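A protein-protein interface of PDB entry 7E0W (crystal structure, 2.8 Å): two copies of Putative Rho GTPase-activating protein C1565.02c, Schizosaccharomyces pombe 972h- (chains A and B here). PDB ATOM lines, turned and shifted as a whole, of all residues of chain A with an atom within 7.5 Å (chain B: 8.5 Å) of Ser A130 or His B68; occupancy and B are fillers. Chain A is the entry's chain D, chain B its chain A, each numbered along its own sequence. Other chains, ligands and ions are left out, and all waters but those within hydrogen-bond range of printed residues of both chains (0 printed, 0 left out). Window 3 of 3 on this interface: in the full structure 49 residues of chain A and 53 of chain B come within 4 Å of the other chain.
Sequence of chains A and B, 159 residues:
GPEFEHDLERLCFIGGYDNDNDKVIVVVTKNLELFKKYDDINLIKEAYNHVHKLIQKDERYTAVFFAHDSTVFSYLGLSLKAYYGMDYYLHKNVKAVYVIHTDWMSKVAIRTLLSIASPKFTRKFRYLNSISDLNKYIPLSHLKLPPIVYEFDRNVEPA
A ring nitrogen (NE2) of His B68 sits at hydrogen-bond distance from the backbone carbonyl oxygen (O) of Asn A129 (3.2 Å).
The backbone carbonyl oxygen (O) of Thr B102 lies close to the side-chain amide oxygen (OD1) of Asn A129 (2.9 Å).
The backbone NH of His B101 is in hydrogen-bond range of the backbone carbonyl oxygen of Leu A128 (2.9 Å).
O of Val B99 is in hydrogen-bond range of N of Leu A128, at 2.9 Å.
NE2 of His B68 sits at hydrogen-bond distance from OG of Ser A130.
The backbone NH of Phe B66 lies within hydrogen-bond range of the backbone carbonyl oxygen of Val B27.
The backbone carbonyl oxygen of Ile B100 is in hydrogen-bond range of the backbone NH of His B68, 3.2 Å away.
The backbone NH (N) of Ala B67 lies within hydrogen-bond range of the backbone carbonyl oxygen (O) of Ile B100 (2.9 Å).
N of Thr B29 sits at hydrogen-bond distance from O of Phe B66 (3.0 Å).
The backbone carbonyl oxygen of Phe B65 lies within hydrogen-bond range of the backbone NH of Ile B100, at 2.7 Å.
The backbone carbonyl oxygen (O) of Ala B67 lies within hydrogen-bond range of a ring nitrogen (ND1) of His B101, 2.5 Å away.
Val B99 touches Tyr A127.
CB of Tyr A127 touches CD2 of Trp B104, 3.4 Å away.
Leu A128 touches Ile B100.
CA of Asn A129 touches O of His B101 (3.8 Å).
Ser A130 touches Ile B100.
Phe B66 touches Ile A131.
Ile A131 touches Ile B100.
Val A149 touches Phe B66 (CG1 to CG, 3.4 Å).
Ser A130 touches just these residues of chain B: His B68 (3.0 Å) and Ile B100 (3.4 Å).
Ala B67 touches none of the printed residues of chain A.
Of the printed residues of chain A, Trp B104 touches Tyr A127 (3.4 Å).
Of the printed residues of chain A, Phe B66 touches Ile A131 and Val A149.
Of the printed residues of chain B, Leu A128 touches Val B99, Ile B100 and His B101.
Printed residues of chain B within 4 Å of Val A149: Phe B66.
Of the printed residues of chain A, Ile B100 touches Leu A128 (3.5 Å), Ser A130 (3.4 Å) and Ile A131 (3.4 Å).
The nearest residue of chain A that does not touch His B68 is Ile A131 (4.4 Å).
Of the 12 printed residues of chain A, 6 touch a printed residue of chain B.
Among the printed residues, no Asp or Glu carboxylate lies within 4 Å of a Lys or Arg side-chain nitrogen of the other chain.
No position is printed for both chains.
Of the 13 pairs that touch across the chains among the printed residues, none has its exchanged pair printed and touching as well.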
ATOM      1  N   TYR A 127     -11.338   8.508  -8.037  1.00  0.00           N
ATOM      2  CA  TYR A 127     -11.370   7.216  -8.708  1.00  0.00           C
ATOM      3  C   TYR A 127     -10.434   6.250  -7.996  1.00  0.00           C
ATOM      4  O   TYR A 127      -9.240   6.531  -7.846  1.00  0.00           O
ATOM      5  CB  TYR A 127     -10.984   7.367 -10.178  1.00  0.00           C
ATOM      6  CG  TYR A 127     -11.903   8.291 -10.942  1.00  0.00           C
ATOM      7  CD1 TYR A 127     -11.795   9.672 -10.820  1.00  0.00           C
ATOM      8  CD2 TYR A 127     -12.889   7.784 -11.775  1.00  0.00           C
ATOM      9  CE1 TYR A 127     -12.639  10.519 -11.511  1.00  0.00           C
ATOM     10  CE2 TYR A 127     -13.737   8.623 -12.471  1.00  0.00           C
ATOM     11  CZ  TYR A 127     -13.608   9.989 -12.336  1.00  0.00           C
ATOM     12  OH  TYR A 127     -14.450  10.830 -13.027  1.00  0.00           O
ATOM     13  N   LEU A 128     -10.978   5.117  -7.563  1.00  0.00           N
ATOM     14  CA  LEU A 128     -10.235   4.120  -6.814  1.00  0.00           C
ATOM     15  C   LEU A 128     -10.090   2.853  -7.647  1.00  0.00           C
ATOM     16  O   LEU A 128     -10.982   2.494  -8.420  1.00  0.00           O
ATOM     17  CB  LEU A 128     -10.938   3.798  -5.494  1.00  0.00           C
ATOM     18  CG  LEU A 128     -11.230   4.956  -4.533  1.00  0.00           C
ATOM     19  CD1 LEU A 128     -11.258   4.441  -3.124  1.00  0.00           C
ATOM     20  CD2 LEU A 128     -10.205   6.077  -4.644  1.00  0.00           C
ATOM     21  N   ASN A 129      -8.954   2.173  -7.478  1.00  0.00           N
ATOM     22  CA  ASN A 129      -8.691   0.976  -8.268  1.00  0.00           C
ATOM     23  C   ASN A 129      -9.536  -0.207  -7.807  1.00  0.00           C
ATOM     24  O   ASN A 129      -9.913  -1.052  -8.628  1.00  0.00           O
ATOM     25  CB  ASN A 129      -7.205   0.627  -8.210  1.00  0.00           C
ATOM     26  CG  ASN A 129      -6.396   1.345  -9.274  1.00  0.00           C
ATOM     27  OD1 ASN A 129      -6.592   1.131 -10.470  1.00  0.00           O
ATOM     28  ND2 ASN A 129      -5.481   2.207  -8.842  1.00  0.00           N
ATOM     29  N   SER A 130      -9.841  -0.292  -6.514  1.00  0.00           N
ATOM     30  CA  SER A 130     -10.666  -1.381  -6.007  1.00  0.00           C
ATOM     31  C   SER A 130     -11.362  -0.932  -4.731  1.00  0.00           C
ATOM     32  O   SER A 130     -11.036   0.106  -4.147  1.00  0.00           O
ATOM     33  CB  SER A 130      -9.839  -2.647  -5.759  1.00  0.00           C
ATOM     34  OG  SER A 130     -10.684  -3.755  -5.497  1.00  0.00           O
ATOM     35  N   ILE A 131     -12.334  -1.743  -4.305  1.00  0.00           N
ATOM     36  CA  ILE A 131     -13.111  -1.453  -3.103  1.00  0.00           C
ATOM     37  C   ILE A 131     -12.215  -1.404  -1.872  1.00  0.00           C
ATOM     38  O   ILE A 131     -12.529  -0.715  -0.892  1.00  0.00           O
ATOM     39  CB  ILE A 131     -14.240  -2.500  -2.959  1.00  0.00           C
ATOM     40  CG1 ILE A 131     -14.881  -2.456  -1.568  1.00  0.00           C
ATOM     41  CG2 ILE A 131     -13.716  -3.895  -3.271  1.00  0.00           C
ATOM     42  CD1 ILE A 131     -16.081  -3.363  -1.418  1.00  0.00           C
ATOM     43  N   SER A 132     -11.080  -2.108  -1.909  1.00  0.00           N
ATOM     44  CA  SER A 132     -10.156  -2.112  -0.778  1.00  0.00           C
ATOM     45  C   SER A 132      -9.726  -0.701  -0.397  1.00  0.00           C
ATOM     46  O   SER A 132      -9.518  -0.404   0.785  1.00  0.00           O
ATOM     47  CB  SER A 132      -8.927  -2.964  -1.109  1.00  0.00           C
ATOM     48  OG  SER A 132      -9.290  -4.163  -1.771  1.00  0.00           O
ATOM     49  N   ASP A 133      -9.596   0.187  -1.386  1.00  0.00           N
ATOM     50  CA  ASP A 133      -9.120   1.540  -1.127  1.00  0.00           C
ATOM     51  C   ASP A 133     -10.200   2.450  -0.553  1.00  0.00           C
ATOM     52  O   ASP A 133      -9.865   3.472   0.058  1.00  0.00           O
ATOM     53  CB  ASP A 133      -8.559   2.156  -2.414  1.00  0.00           C
ATOM     54  CG  ASP A 133      -7.630   1.212  -3.161  1.00  0.00           C
ATOM     55  OD1 ASP A 133      -7.994   0.028  -3.334  1.00  0.00           O
ATOM     56  OD2 ASP A 133      -6.538   1.653  -3.582  1.00  0.00           O
ATOM     57  N   LEU A 134     -11.482   2.112  -0.729  1.00  0.00           N
ATOM     58  CA  LEU A 134     -12.546   2.986  -0.243  1.00  0.00           C
ATOM     59  C   LEU A 134     -12.549   3.061   1.279  1.00  0.00           C
ATOM     60  O   LEU A 134     -12.858   4.118   1.842  1.00  0.00           O
ATOM     61  CB  LEU A 134     -13.900   2.497  -0.784  1.00  0.00           C
ATOM     62  CG  LEU A 134     -15.136   3.410  -0.844  1.00  0.00           C
ATOM     63  CD1 LEU A 134     -16.285   2.699  -1.540  1.00  0.00           C
ATOM     64  CD2 LEU A 134     -15.593   3.884   0.518  1.00  0.00           C
ATOM     65  N   ASN A 135     -12.143   1.974   1.948  1.00  0.00           N
ATOM     66  CA  ASN A 135     -12.184   1.905   3.407  1.00  0.00           C
ATOM     67  C   ASN A 135     -11.501   3.100   4.061  1.00  0.00           C
ATOM     68  O   ASN A 135     -11.819   3.448   5.204  1.00  0.00           O
ATOM     69  CB  ASN A 135     -11.532   0.605   3.879  1.00  0.00           C
ATOM     70  CG  ASN A 135     -12.161   0.063   5.147  1.00  0.00           C
ATOM     71  OD1 ASN A 135     -13.228   0.509   5.564  1.00  0.00           O
ATOM     72  ND2 ASN A 135     -11.496  -0.903   5.773  1.00  0.00           N
ATOM     73  N   ILE A 148     -21.487  -9.208  -5.044  1.00  0.00           N
ATOM     74  CA  ILE A 148     -20.827  -8.979  -6.328  1.00  0.00           C
ATOM     75  C   ILE A 148     -19.681  -7.983  -6.193  1.00  0.00           C
ATOM     76  O   ILE A 148     -18.692  -8.063  -6.930  1.00  0.00           O
ATOM     77  CB  ILE A 148     -21.859  -8.519  -7.378  1.00  0.00           C
ATOM     78  CG1 ILE A 148     -22.973  -9.558  -7.524  1.00  0.00           C
ATOM     79  CG2 ILE A 148     -21.202  -8.274  -8.733  1.00  0.00           C
ATOM     80  CD1 ILE A 148     -24.213  -9.256  -6.709  1.00  0.00           C
ATOM     81  N   VAL A 149     -19.778  -7.042  -5.248  1.00  0.00           N
ATOM     82  CA  VAL A 149     -18.699  -6.071  -5.065  1.00  0.00           C
ATOM     83  C   VAL A 149     -17.468  -6.688  -4.421  1.00  0.00           C
ATOM     84  O   VAL A 149     -16.483  -5.977  -4.182  1.00  0.00           O
ATOM     85  CB  VAL A 149     -19.136  -4.872  -4.198  1.00  0.00           C
ATOM     86  CG1 VAL A 149     -20.153  -4.003  -4.944  1.00  0.00           C
ATOM     87  CG2 VAL A 149     -19.666  -5.352  -2.881  1.00  0.00           C
ATOM     88  N   GLU A 151     -16.400 -10.129  -5.461  1.00  0.00           N
ATOM     89  CA  GLU A 151     -15.962 -11.258  -6.282  1.00  0.00           C
ATOM     90  C   GLU A 151     -14.596 -11.002  -6.916  1.00  0.00           C
ATOM     91  O   GLU A 151     -13.895 -10.058  -6.551  1.00  0.00           O
ATOM     92  CB  GLU A 151     -16.994 -11.555  -7.359  1.00  0.00           C
ATOM     93  N   VAL B  27     -24.537   2.674  -5.973  1.00  0.00           N
ATOM     94  CA  VAL B  27     -25.055   2.226  -7.260  1.00  0.00           C
ATOM     95  C   VAL B  27     -24.079   1.203  -7.804  1.00  0.00           C
ATOM     96  O   VAL B  27     -22.875   1.470  -7.903  1.00  0.00           O
ATOM     97  CB  VAL B  27     -25.252   3.390  -8.245  1.00  0.00           C
ATOM     98  CG1 VAL B  27     -24.017   4.274  -8.280  1.00  0.00           C
ATOM     99  CG2 VAL B  27     -25.564   2.850  -9.631  1.00  0.00           C
ATOM    100  N   VAL B  28     -24.582   0.030  -8.126  1.00  0.00           N
ATOM    101  CA  VAL B  28     -23.788  -1.064  -8.655  1.00  0.00           C
ATOM    102  C   VAL B  28     -23.893  -1.033 -10.181  1.00  0.00           C
ATOM    103  O   VAL B  28     -24.995  -1.049 -10.736  1.00  0.00           O
ATOM    104  CB  VAL B  28     -24.242  -2.402  -8.041  1.00  0.00           C
ATOM    105  CG1 VAL B  28     -23.888  -2.405  -6.544  1.00  0.00           C
ATOM    106  CG2 VAL B  28     -25.778  -2.580  -8.177  1.00  0.00           C
ATOM    107  N   THR B  29     -22.750  -0.933 -10.870  1.00  0.00           N
ATOM    108  CA  THR B  29     -22.833  -0.752 -12.322  1.00  0.00           C
ATOM    109  C   THR B  29     -23.032  -2.068 -13.061  1.00  0.00           C
ATOM    110  O   THR B  29     -23.532  -2.066 -14.186  1.00  0.00           O
ATOM    111  CB  THR B  29     -21.603  -0.028 -12.863  1.00  0.00           C
ATOM    112  OG1 THR B  29     -20.525  -0.955 -13.046  1.00  0.00           O
ATOM    113  CG2 THR B  29     -21.157   1.116 -11.941  1.00  0.00           C
ATOM    114  N   LYS B  30     -22.655  -3.199 -12.467  1.00  0.00           N
ATOM    115  CA  LYS B  30     -22.922  -4.469 -13.127  1.00  0.00           C
ATOM    116  C   LYS B  30     -24.393  -4.810 -13.232  1.00  0.00           C
ATOM    117  O   LYS B  30     -24.741  -5.813 -13.870  1.00  0.00           O
ATOM    118  N   PHE B  65     -19.869   4.503  -6.821  1.00  0.00           N
ATOM    119  CA  PHE B  65     -20.107   3.738  -8.042  1.00  0.00           C
ATOM    120  C   PHE B  65     -19.201   2.513  -8.040  1.00  0.00           C
ATOM    121  O   PHE B  65     -17.979   2.647  -7.927  1.00  0.00           O
ATOM    122  CB  PHE B  65     -19.849   4.593  -9.285  1.00  0.00           C
ATOM    123  CG  PHE B  65     -20.849   5.702  -9.486  1.00  0.00           C
ATOM    124  CD1 PHE B  65     -20.819   6.835  -8.689  1.00  0.00           C
ATOM    125  CD2 PHE B  65     -21.804   5.619 -10.485  1.00  0.00           C
ATOM    126  CE1 PHE B  65     -21.735   7.855  -8.874  1.00  0.00           C
ATOM    127  CE2 PHE B  65     -22.721   6.635 -10.675  1.00  0.00           C
ATOM    128  CZ  PHE B  65     -22.686   7.754  -9.869  1.00  0.00           C
ATOM    129  N   PHE B  66     -19.795   1.327  -8.169  1.00  0.00           N
ATOM    130  CA  PHE B  66     -19.051   0.070  -8.166  1.00  0.00           C
ATOM    131  C   PHE B  66     -18.944  -0.456  -9.596  1.00  0.00           C
ATOM    132  O   PHE B  66     -19.897  -1.035 -10.126  1.00  0.00           O
ATOM    133  CB  PHE B  66     -19.721  -0.950  -7.248  1.00  0.00           C
ATOM    134  CG  PHE B  66     -19.294  -0.841  -5.809  1.00  0.00           C
ATOM    135  CD1 PHE B  66     -18.046  -1.290  -5.410  1.00  0.00           C
ATOM    136  CD2 PHE B  66     -20.137  -0.289  -4.858  1.00  0.00           C
ATOM    137  CE1 PHE B  66     -17.645  -1.192  -4.091  1.00  0.00           C
ATOM    138  CE2 PHE B  66     -19.741  -0.186  -3.536  1.00  0.00           C
ATOM    139  CZ  PHE B  66     -18.492  -0.637  -3.154  1.00  0.00           C
ATOM    140  N   ALA B  67     -17.772  -0.279 -10.205  1.00  0.00           N
ATOM    141  CA  ALA B  67     -17.552  -0.630 -11.598  1.00  0.00           C
ATOM    142  C   ALA B  67     -16.322  -1.483 -11.852  1.00  0.00           C
ATOM    143  O   ALA B  67     -15.616  -1.276 -12.844  1.00  0.00           O
ATOM    144  N   HIS B  68     -16.048  -2.439 -10.967  1.00  0.00           N
ATOM    145  CA  HIS B  68     -14.784  -3.166 -10.970  1.00  0.00           C
ATOM    146  C   HIS B  68     -14.731  -4.332 -11.957  1.00  0.00           C
ATOM    147  O   HIS B  68     -13.702  -5.015 -12.019  1.00  0.00           O
ATOM    148  CB  HIS B  68     -14.481  -3.689  -9.562  1.00  0.00           C
ATOM    149  CG  HIS B  68     -13.022  -3.898  -9.303  1.00  0.00           C
ATOM    150  ND1 HIS B  68     -12.147  -4.320 -10.280  1.00  0.00           N
ATOM    151  CD2 HIS B  68     -12.282  -3.732  -8.182  1.00  0.00           C
ATOM    152  CE1 HIS B  68     -10.931  -4.410  -9.771  1.00  0.00           C
ATOM    153  NE2 HIS B  68     -10.986  -4.058  -8.499  1.00  0.00           N
ATOM    154  N   ASP B  69     -15.784  -4.583 -12.729  1.00  0.00           N
ATOM    155  CA  ASP B  69     -15.791  -5.723 -13.635  1.00  0.00           C
ATOM    156  C   ASP B  69     -15.210  -5.323 -14.992  1.00  0.00           C
ATOM    157  O   ASP B  69     -14.623  -4.250 -15.151  1.00  0.00           O
ATOM    158  CB  ASP B  69     -17.204  -6.288 -13.762  1.00  0.00           C
ATOM    159  CG  ASP B  69     -17.797  -6.673 -12.422  1.00  0.00           C
ATOM    160  OD1 ASP B  69     -17.607  -5.914 -11.448  1.00  0.00           O
ATOM    161  OD2 ASP B  69     -18.444  -7.738 -12.343  1.00  0.00           O
ATOM    162  N   SER B  70     -15.355  -6.202 -15.985  1.00  0.00           N
ATOM    163  CA  SER B  70     -14.864  -5.927 -17.322  1.00  0.00           C
ATOM    164  C   SER B  70     -15.782  -6.433 -18.417  1.00  0.00           C
ATOM    165  O   SER B  70     -16.993  -6.566 -18.211  1.00  0.00           O
ATOM    166  N   THR B  71     -15.219  -6.718 -19.585  1.00  0.00           N
ATOM    167  CA  THR B  71     -16.009  -7.182 -20.707  1.00  0.00           C
ATOM    168  C   THR B  71     -16.521  -6.049 -21.572  1.00  0.00           C
ATOM    169  O   THR B  71     -16.103  -4.891 -21.469  1.00  0.00           O
ATOM    170  N   SER B  74     -18.672  -1.761 -18.976  1.00  0.00           N
ATOM    171  CA  SER B  74     -18.884  -1.830 -17.538  1.00  0.00           C
ATOM    172  C   SER B  74     -19.969  -0.866 -17.086  1.00  0.00           C
ATOM    173  O   SER B  74     -20.305  -0.839 -15.894  1.00  0.00           O
ATOM    174  CB  SER B  74     -17.577  -1.540 -16.785  1.00  0.00           C
ATOM    175  N   LEU B  76     -20.230   1.981 -16.230  1.00  0.00           N
ATOM    176  CA  LEU B  76     -19.883   3.133 -15.409  1.00  0.00           C
ATOM    177  C   LEU B  76     -20.081   4.416 -16.204  1.00  0.00           C
ATOM    178  O   LEU B  76     -20.713   5.365 -15.729  1.00  0.00           O
ATOM    179  CB  LEU B  76     -18.439   2.989 -14.927  1.00  0.00           C
ATOM    180  CG  LEU B  76     -17.826   3.763 -13.759  1.00  0.00           C
ATOM    181  CD1 LEU B  76     -16.403   3.252 -13.556  1.00  0.00           C
ATOM    182  CD2 LEU B  76     -17.848   5.287 -13.916  1.00  0.00           C
ATOM    183  N   TYR B  98     -17.214   8.653  -5.050  1.00  0.00           N
ATOM    184  CA  TYR B  98     -16.197   7.623  -5.181  1.00  0.00           C
ATOM    185  C   TYR B  98     -16.610   6.644  -6.270  1.00  0.00           C
ATOM    186  O   TYR B  98     -17.775   6.247  -6.359  1.00  0.00           O
ATOM    187  CB  TYR B  98     -15.984   6.894  -3.854  1.00  0.00           C
ATOM    188  CG  TYR B  98     -15.578   7.823  -2.737  1.00  0.00           C
ATOM    189  CD1 TYR B  98     -14.253   8.206  -2.573  1.00  0.00           C
ATOM    190  CD2 TYR B  98     -16.520   8.333  -1.857  1.00  0.00           C
ATOM    191  CE1 TYR B  98     -13.878   9.065  -1.558  1.00  0.00           C
ATOM    192  CE2 TYR B  98     -16.155   9.191  -0.839  1.00  0.00           C
ATOM    193  CZ  TYR B  98     -14.834   9.555  -0.694  1.00  0.00           C
ATOM    194  OH  TYR B  98     -14.470  10.411   0.321  1.00  0.00           O
ATOM    195  N   VAL B  99     -15.649   6.270  -7.109  1.00  0.00           N
ATOM    196  CA  VAL B  99     -15.908   5.465  -8.296  1.00  0.00           C
ATOM    197  C   VAL B  99     -14.871   4.351  -8.342  1.00  0.00           C
ATOM    198  O   VAL B  99     -13.674   4.620  -8.473  1.00  0.00           O
ATOM    199  CB  VAL B  99     -15.863   6.311  -9.580  1.00  0.00           C
ATOM    200  CG1 VAL B  99     -15.845   5.419 -10.807  1.00  0.00           C
ATOM    201  CG2 VAL B  99     -17.051   7.263  -9.624  1.00  0.00           C
ATOM    202  N   ILE B 100     -15.334   3.110  -8.243  1.00  0.00           N
ATOM    203  CA  ILE B 100     -14.453   1.956  -8.069  1.00  0.00           C
ATOM    204  C   ILE B 100     -14.268   1.311  -9.440  1.00  0.00           C
ATOM    205  O   ILE B 100     -15.018   0.420  -9.845  1.00  0.00           O
ATOM    206  CB  ILE B 100     -15.011   0.973  -7.040  1.00  0.00           C
ATOM    207  CG1 ILE B 100     -15.407   1.709  -5.755  1.00  0.00           C
ATOM    208  CG2 ILE B 100     -14.001  -0.117  -6.744  1.00  0.00           C
ATOM    209  CD1 ILE B 100     -14.293   2.533  -5.137  1.00  0.00           C
ATOM    210  N   HIS B 101     -13.236   1.755 -10.158  1.00  0.00           N
ATOM    211  CA  HIS B 101     -12.831   1.159 -11.425  1.00  0.00           C
ATOM    212  C   HIS B 101     -11.318   1.262 -11.549  1.00  0.00           C
ATOM    213  O   HIS B 101     -10.728   2.276 -11.168  1.00  0.00           O
ATOM    214  CB  HIS B 101     -13.499   1.847 -12.620  1.00  0.00           C
ATOM    215  CG  HIS B 101     -13.566   0.998 -13.852  1.00  0.00           C
ATOM    216  ND1 HIS B 101     -13.495  -0.378 -13.813  1.00  0.00           N
ATOM    217  CD2 HIS B 101     -13.695   1.330 -15.158  1.00  0.00           C
ATOM    218  CE1 HIS B 101     -13.576  -0.856 -15.041  1.00  0.00           C
ATOM    219  NE2 HIS B 101     -13.698   0.160 -15.877  1.00  0.00           N
ATOM    220  N   THR B 102     -10.695   0.215 -12.094  1.00  0.00           N
ATOM    221  CA  THR B 102      -9.236   0.159 -12.110  1.00  0.00           C
ATOM    222  C   THR B 102      -8.653   0.983 -13.256  1.00  0.00           C
ATOM    223  O   THR B 102      -7.842   1.888 -13.030  1.00  0.00           O
ATOM    224  CB  THR B 102      -8.759  -1.300 -12.172  1.00  0.00           C
ATOM    225  OG1 THR B 102      -7.364  -1.340 -12.501  1.00  0.00           O
ATOM    226  CG2 THR B 102      -9.558  -2.110 -13.191  1.00  0.00           C
ATOM    227  N   ASP B 103      -9.051   0.689 -14.494  1.00  0.00           N
ATOM    228  CA  ASP B 103      -8.625   1.481 -15.647  1.00  0.00           C
ATOM    229  C   ASP B 103      -9.711   2.502 -15.993  1.00  0.00           C
ATOM    230  O   ASP B 103     -10.340   2.473 -17.050  1.00  0.00           O
ATOM    231  CB  ASP B 103      -8.287   0.570 -16.827  1.00  0.00           C
ATOM    232  CG  ASP B 103      -9.467  -0.270 -17.287  1.00  0.00           C
ATOM    233  OD1 ASP B 103     -10.315  -0.631 -16.444  1.00  0.00           O
ATOM    234  OD2 ASP B 103      -9.545  -0.569 -18.498  1.00  0.00           O
ATOM    235  N   TRP B 104      -9.907   3.436 -15.059  1.00  0.00           N
ATOM    236  CA  TRP B 104     -10.979   4.418 -15.188  1.00  0.00           C
ATOM    237  C   TRP B 104     -10.647   5.515 -16.192  1.00  0.00           C
ATOM    238  O   TRP B 104     -11.560   6.092 -16.792  1.00  0.00           O
ATOM    239  CB  TRP B 104     -11.290   5.036 -13.824  1.00  0.00           C
ATOM    240  CG  TRP B 104     -10.070   5.501 -13.093  1.00  0.00           C
ATOM    241  CD1 TRP B 104      -9.315   4.779 -12.216  1.00  0.00           C
ATOM    242  CD2 TRP B 104      -9.461   6.795 -13.174  1.00  0.00           C
ATOM    243  NE1 TRP B 104      -8.273   5.541 -11.747  1.00  0.00           N
ATOM    244  CE2 TRP B 104      -8.340   6.785 -12.320  1.00  0.00           C
ATOM    245  CE3 TRP B 104      -9.755   7.964 -13.885  1.00  0.00           C
ATOM    246  CZ2 TRP B 104      -7.513   7.894 -12.159  1.00  0.00           C
ATOM    247  CZ3 TRP B 104      -8.933   9.064 -13.724  1.00  0.00           C
ATOM    248  CH2 TRP B 104      -7.825   9.022 -12.868  1.00  0.00           C
